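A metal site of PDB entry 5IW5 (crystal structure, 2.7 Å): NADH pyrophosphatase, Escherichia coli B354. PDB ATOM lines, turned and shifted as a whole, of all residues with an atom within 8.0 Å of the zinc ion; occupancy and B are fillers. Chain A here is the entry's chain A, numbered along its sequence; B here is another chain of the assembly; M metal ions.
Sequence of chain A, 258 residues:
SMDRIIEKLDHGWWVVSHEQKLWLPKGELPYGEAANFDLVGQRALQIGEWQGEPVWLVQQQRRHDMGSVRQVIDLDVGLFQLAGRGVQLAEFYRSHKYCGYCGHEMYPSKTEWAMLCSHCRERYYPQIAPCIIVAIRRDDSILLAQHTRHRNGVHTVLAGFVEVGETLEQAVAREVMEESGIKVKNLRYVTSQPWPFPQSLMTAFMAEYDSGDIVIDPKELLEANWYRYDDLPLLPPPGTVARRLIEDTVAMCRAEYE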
ATOM      1  N   TYR A  98      27.433  -7.886 -25.154  1.00  0.00           N
ATOM      2  CA  TYR A  98      26.745  -6.617 -24.955  1.00  0.00           C
ATOM      3  C   TYR A  98      26.245  -6.614 -23.580  1.00  0.00           C
ATOM      4  O   TYR A  98      25.946  -7.634 -23.035  1.00  0.00           O
ATOM      5  CB  TYR A  98      25.566  -6.450 -25.867  1.00  0.00           C
ATOM      6  CG  TYR A  98      25.910  -6.540 -27.294  1.00  0.00           C
ATOM      7  CD1 TYR A  98      26.567  -5.521 -27.951  1.00  0.00           C
ATOM      8  CD2 TYR A  98      25.574  -7.640 -28.011  1.00  0.00           C
ATOM      9  CE1 TYR A  98      26.877  -5.618 -29.259  1.00  0.00           C
ATOM     10  CE2 TYR A  98      25.863  -7.732 -29.323  1.00  0.00           C
ATOM     11  CZ  TYR A  98      26.515  -6.732 -29.943  1.00  0.00           C
ATOM     12  OH  TYR A  98      26.785  -6.896 -31.262  1.00  0.00           O
ATOM     13  N   CYS A  99      26.196  -5.432 -23.010  1.00  0.00           N
ATOM     14  CA  CYS A  99      25.778  -5.243 -21.658  1.00  0.00           C
ATOM     15  C   CYS A  99      24.287  -5.341 -21.502  1.00  0.00           C
ATOM     16  O   CYS A  99      23.540  -4.725 -22.180  1.00  0.00           O
ATOM     17  CB  CYS A  99      26.233  -3.900 -21.202  1.00  0.00           C
ATOM     18  SG  CYS A  99      25.733  -3.463 -19.577  1.00  0.00           S
ATOM     19  N   GLY A 100      23.886  -6.148 -20.550  1.00  0.00           N
ATOM     20  CA  GLY A 100      22.510  -6.324 -20.240  1.00  0.00           C
ATOM     21  C   GLY A 100      21.874  -5.098 -19.737  1.00  0.00           C
ATOM     22  O   GLY A 100      20.740  -4.885 -19.943  1.00  0.00           O
ATOM     23  N   TYR A 101      22.600  -4.320 -18.979  1.00  0.00           N
ATOM     24  CA  TYR A 101      22.156  -3.010 -18.608  1.00  0.00           C
ATOM     25  C   TYR A 101      22.021  -1.903 -19.651  1.00  0.00           C
ATOM     26  O   TYR A 101      20.990  -1.304 -19.747  1.00  0.00           O
ATOM     27  CB  TYR A 101      23.127  -2.519 -17.591  1.00  0.00           C
ATOM     28  CG  TYR A 101      23.282  -3.411 -16.429  1.00  0.00           C
ATOM     29  CD1 TYR A 101      24.253  -4.357 -16.402  1.00  0.00           C
ATOM     30  CD2 TYR A 101      22.499  -3.267 -15.326  1.00  0.00           C
ATOM     31  CE1 TYR A 101      24.417  -5.169 -15.303  1.00  0.00           C
ATOM     32  CE2 TYR A 101      22.672  -4.063 -14.230  1.00  0.00           C
ATOM     33  CZ  TYR A 101      23.637  -5.012 -14.244  1.00  0.00           C
ATOM     34  OH  TYR A 101      23.815  -5.768 -13.180  1.00  0.00           O
ATOM     35  N   CYS A 102      23.034  -1.645 -20.462  1.00  0.00           N
ATOM     36  CA  CYS A 102      23.015  -0.527 -21.393  1.00  0.00           C
ATOM     37  C   CYS A 102      22.983  -0.887 -22.823  1.00  0.00           C
ATOM     38  O   CYS A 102      22.866  -0.028 -23.645  1.00  0.00           O
ATOM     39  CB  CYS A 102      24.196   0.407 -21.257  1.00  0.00           C
ATOM     40  SG  CYS A 102      25.448  -0.082 -20.104  1.00  0.00           S
ATOM     41  N   GLY A 103      23.131  -2.156 -23.136  1.00  0.00           N
ATOM     42  CA  GLY A 103      22.981  -2.636 -24.492  1.00  0.00           C
ATOM     43  C   GLY A 103      24.213  -2.386 -25.331  1.00  0.00           C
ATOM     44  O   GLY A 103      24.247  -2.741 -26.499  1.00  0.00           O
ATOM     45  N   HIS A 104      25.214  -1.763 -24.728  1.00  0.00           N
ATOM     46  CA  HIS A 104      26.454  -1.410 -25.411  1.00  0.00           C
ATOM     47  C   HIS A 104      27.535  -2.465 -25.270  1.00  0.00           C
ATOM     48  O   HIS A 104      27.525  -3.236 -24.323  1.00  0.00           O
ATOM     49  CB  HIS A 104      26.979  -0.119 -24.825  1.00  0.00           C
ATOM     50  CG  HIS A 104      26.270   1.106 -25.307  1.00  0.00           C
ATOM     51  ND1 HIS A 104      26.880   2.044 -26.109  1.00  0.00           N
ATOM     52  CD2 HIS A 104      25.002   1.537 -25.109  1.00  0.00           C
ATOM     53  CE1 HIS A 104      26.015   3.000 -26.387  1.00  0.00           C
ATOM     54  NE2 HIS A 104      24.874   2.724 -25.787  1.00  0.00           N
ATOM     55  N   GLU A 105      28.489  -2.479 -26.204  1.00  0.00           N
ATOM     56  CA  GLU A 105      29.530  -3.495 -26.196  1.00  0.00           C
ATOM     57  C   GLU A 105      30.385  -3.426 -24.943  1.00  0.00           C
ATOM     58  O   GLU A 105      30.777  -2.326 -24.490  1.00  0.00           O
ATOM     59  CB  GLU A 105      30.396  -3.456 -27.473  1.00  0.00           C
ATOM     60  CG  GLU A 105      29.710  -4.020 -28.709  1.00  0.00           C
ATOM     61  CD  GLU A 105      30.366  -3.552 -30.015  1.00  0.00           C
ATOM     62  OE1 GLU A 105      31.540  -3.150 -29.985  1.00  0.00           O
ATOM     63  OE2 GLU A 105      29.698  -3.580 -31.075  1.00  0.00           O
ATOM     64  N   MET A 106      30.641  -4.592 -24.362  1.00  0.00           N
ATOM     65  CA  MET A 106      31.480  -4.691 -23.187  1.00  0.00           C
ATOM     66  C   MET A 106      32.853  -5.114 -23.650  1.00  0.00           C
ATOM     67  O   MET A 106      33.014  -5.637 -24.744  1.00  0.00           O
ATOM     68  CB  MET A 106      30.935  -5.745 -22.228  1.00  0.00           C
ATOM     69  CG  MET A 106      29.519  -5.472 -21.742  1.00  0.00           C
ATOM     70  SD  MET A 106      28.972  -6.625 -20.454  1.00  0.00           S
ATOM     71  CE  MET A 106      29.759  -5.881 -19.023  1.00  0.00           C
ATOM     72  N   MET A 115      33.571  -9.024 -17.232  1.00  0.00           N
ATOM     73  CA  MET A 115      33.265  -8.140 -18.323  1.00  0.00           C
ATOM     74  C   MET A 115      32.860  -6.766 -17.876  1.00  0.00           C
ATOM     75  O   MET A 115      32.034  -6.624 -17.010  1.00  0.00           O
ATOM     76  CB  MET A 115      32.159  -8.732 -19.165  1.00  0.00           C
ATOM     77  CG  MET A 115      32.577  -9.863 -20.060  1.00  0.00           C
ATOM     78  SD  MET A 115      33.444  -9.375 -21.517  1.00  0.00           S
ATOM     79  CE  MET A 115      32.111  -8.963 -22.618  1.00  0.00           C
ATOM     80  N   LEU A 116      33.430  -5.741 -18.501  1.00  0.00           N
ATOM     81  CA  LEU A 116      33.226  -4.343 -18.132  1.00  0.00           C
ATOM     82  C   LEU A 116      32.571  -3.579 -19.218  1.00  0.00           C
ATOM     83  O   LEU A 116      32.900  -3.748 -20.324  1.00  0.00           O
ATOM     84  CB  LEU A 116      34.554  -3.732 -17.807  1.00  0.00           C
ATOM     85  CG  LEU A 116      35.420  -4.654 -16.989  1.00  0.00           C
ATOM     86  CD1 LEU A 116      36.815  -4.141 -16.788  1.00  0.00           C
ATOM     87  CD2 LEU A 116      34.768  -4.938 -15.681  1.00  0.00           C
ATOM     88  N   CYS A 117      31.568  -2.783 -18.916  1.00  0.00           N
ATOM     89  CA  CYS A 117      30.830  -2.047 -19.947  1.00  0.00           C
ATOM     90  C   CYS A 117      31.491  -0.953 -20.782  1.00  0.00           C
ATOM     91  O   CYS A 117      31.416  -0.990 -22.013  1.00  0.00           O
ATOM     92  CB  CYS A 117      29.651  -1.388 -19.334  1.00  0.00           C
ATOM     93  SG  CYS A 117      28.555  -0.901 -20.607  1.00  0.00           S
ATOM     94  N   SER A 118      32.158  -0.028 -20.126  1.00  0.00           N
ATOM     95  CA  SER A 118      32.723   1.160 -20.754  1.00  0.00           C
ATOM     96  C   SER A 118      31.714   2.278 -20.945  1.00  0.00           C
ATOM     97  O   SER A 118      32.074   3.368 -21.317  1.00  0.00           O
ATOM     98  CB  SER A 118      33.367   0.867 -22.100  1.00  0.00           C
ATOM     99  OG  SER A 118      32.446   0.265 -22.994  1.00  0.00           O
ATOM    100  N   HIS A 119      30.455   2.012 -20.680  1.00  0.00           N
ATOM    101  CA  HIS A 119      29.478   3.046 -20.655  1.00  0.00           C
ATOM    102  C   HIS A 119      28.949   3.310 -19.286  1.00  0.00           C
ATOM    103  O   HIS A 119      28.649   4.433 -18.943  1.00  0.00           O
ATOM    104  CB  HIS A 119      28.384   2.751 -21.639  1.00  0.00           C
ATOM    105  CG  HIS A 119      28.594   3.488 -22.904  1.00  0.00           C
ATOM    106  ND1 HIS A 119      29.606   3.161 -23.775  1.00  0.00           N
ATOM    107  CD2 HIS A 119      28.042   4.629 -23.365  1.00  0.00           C
ATOM    108  CE1 HIS A 119      29.615   4.021 -24.779  1.00  0.00           C
ATOM    109  NE2 HIS A 119      28.669   4.919 -24.556  1.00  0.00           N
ATOM    110  N   CYS A 120      28.938   2.282 -18.486  1.00  0.00           N
ATOM    111  CA  CYS A 120      28.513   2.320 -17.144  1.00  0.00           C
ATOM    112  C   CYS A 120      29.440   1.389 -16.398  1.00  0.00           C
ATOM    113  O   CYS A 120      30.101   0.598 -16.990  1.00  0.00           O
ATOM    114  CB  CYS A 120      27.083   1.873 -17.066  1.00  0.00           C
ATOM    115  SG  CYS A 120      26.954   0.121 -17.223  1.00  0.00           S
ATOM    116  N   ARG A 121      29.471   1.499 -15.108  1.00  0.00           N
ATOM    117  CA  ARG A 121      30.466   0.843 -14.317  1.00  0.00           C
ATOM    118  C   ARG A 121      29.889  -0.471 -13.879  1.00  0.00           C
ATOM    119  O   ARG A 121      30.279  -1.091 -12.931  1.00  0.00           O
ATOM    120  CB  ARG A 121      30.887   1.694 -13.108  1.00  0.00           C
ATOM    121  CG  ARG A 121      31.657   2.956 -13.475  1.00  0.00           C
ATOM    122  CD  ARG A 121      32.108   3.771 -12.275  1.00  0.00           C
ATOM    123  NE  ARG A 121      32.785   5.000 -12.670  1.00  0.00           N
ATOM    124  CZ  ARG A 121      33.173   5.946 -11.828  1.00  0.00           C
ATOM    125  NH1 ARG A 121      32.960   5.806 -10.532  1.00  0.00           N
ATOM    126  NH2 ARG A 121      33.785   7.034 -12.284  1.00  0.00           N
ATOM    127  N   GLU A 122      28.922  -0.903 -14.629  1.00  0.00           N
ATOM    128  CA  GLU A 122      28.314  -2.177 -14.340  1.00  0.00           C
ATOM    129  C   GLU A 122      29.196  -3.272 -14.927  1.00  0.00           C
ATOM    130  O   GLU A 122      29.861  -3.075 -15.937  1.00  0.00           O
ATOM    131  CB  GLU A 122      26.912  -2.205 -14.930  1.00  0.00           C
ATOM    132  CG  GLU A 122      25.852  -2.706 -14.003  1.00  0.00           C
ATOM    133  CD  GLU A 122      25.606  -1.839 -12.792  1.00  0.00           C
ATOM    134  OE1 GLU A 122      24.901  -0.803 -12.918  1.00  0.00           O
ATOM    135  OE2 GLU A 122      26.108  -2.205 -11.705  1.00  0.00           O
ATOM    136  N   ARG A 123      29.229  -4.435 -14.280  1.00  0.00           N
ATOM    137  CA  ARG A 123      30.068  -5.545 -14.740  1.00  0.00           C
ATOM    138  C   ARG A 123      29.412  -6.897 -14.525  1.00  0.00           C
ATOM    139  O   ARG A 123      28.343  -6.994 -13.939  1.00  0.00           O
ATOM    140  CB  ARG A 123      31.447  -5.500 -14.091  1.00  0.00           C
ATOM    141  CG  ARG A 123      31.450  -5.090 -12.639  1.00  0.00           C
ATOM    142  CD  ARG A 123      32.864  -5.008 -12.097  1.00  0.00           C
ATOM    143  NE  ARG A 123      33.623  -3.886 -12.653  1.00  0.00           N
ATOM    144  CZ  ARG A 123      34.846  -3.567 -12.273  1.00  0.00           C
ATOM    145  NH1 ARG A 123      35.450  -4.279 -11.334  1.00  0.00           N
ATOM    146  NH2 ARG A 123      35.475  -2.535 -12.835  1.00  0.00           N
ATOM    147  N   TYR A 124      30.072  -7.938 -15.029  1.00  0.00           N
ATOM    148  CA  TYR A 124      29.605  -9.317 -14.909  1.00  0.00           C
ATOM    149  C   TYR A 124      30.706 -10.280 -14.447  1.00  0.00           C
ATOM    150  O   TYR A 124      31.871 -10.113 -14.757  1.00  0.00           O
ATOM    151  CB  TYR A 124      29.015  -9.806 -16.241  1.00  0.00           C
ATOM    152  CG  TYR A 124      27.696  -9.184 -16.593  1.00  0.00           C
ATOM    153  CD1 TYR A 124      27.601  -8.132 -17.502  1.00  0.00           C
ATOM    154  CD2 TYR A 124      26.526  -9.648 -16.019  1.00  0.00           C
ATOM    155  CE1 TYR A 124      26.379  -7.568 -17.827  1.00  0.00           C
ATOM    156  CE2 TYR A 124      25.306  -9.098 -16.329  1.00  0.00           C
ATOM    157  CZ  TYR A 124      25.233  -8.058 -17.226  1.00  0.00           C
ATOM    158  OH  TYR A 124      24.006  -7.521 -17.520  1.00  0.00           O
ATOM    159  N   TYR B  98      18.973  -5.914 -22.032  1.00  0.00           N
ATOM    160  CA  TYR B  98      19.474  -6.178 -23.383  1.00  0.00           C
ATOM    161  C   TYR B  98      20.206  -7.443 -23.331  1.00  0.00           C
ATOM    162  O   TYR B  98      20.757  -7.784 -22.323  1.00  0.00           O
ATOM    163  CB  TYR B  98      20.428  -5.113 -23.847  1.00  0.00           C
ATOM    164  CG  TYR B  98      19.852  -3.760 -23.847  1.00  0.00           C
ATOM    165  CD1 TYR B  98      18.934  -3.359 -24.796  1.00  0.00           C
ATOM    166  CD2 TYR B  98      20.224  -2.865 -22.914  1.00  0.00           C
ATOM    167  CE1 TYR B  98      18.413  -2.116 -24.781  1.00  0.00           C
ATOM    168  CE2 TYR B  98      19.723  -1.607 -22.903  1.00  0.00           C
ATOM    169  CZ  TYR B  98      18.819  -1.240 -23.830  1.00  0.00           C
ATOM    170  OH  TYR B  98      18.345   0.030 -23.759  1.00  0.00           O
HETATM  171 ZN    ZN M   1      26.807  -1.132 -19.478  1.00  0.00          ZN
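The zinc ion is bound by SG of Cys 102 (1.8 Å), SG of Cys 117 (2.1 Å), SG of Cys 99 (2.6 Å) and SG of Cys 120 (2.6 Å).
The backbone carbonyl oxygen (O) of His 104 is in hydrogen-bond range of the backbone NH (N) of Cys 99. The backbone NH of Glu 122 lies close to the side-chain sulfur of Cys 120 (3.4 Å). The side-chain sulfur (SG) of Cys 99 sits close to the backbone NH (N) of Tyr 101, at 3.3 Å. N of His 119 lies close to SG of Cys 117. The backbone carbonyl oxygen (O) of Glu 122 sits at hydrogen-bond distance from the backbone NH (N) of Cys 117.
Within 4 Å of the zinc ion: Cys 99, Cys 102, Cys 117 and Cys 120.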
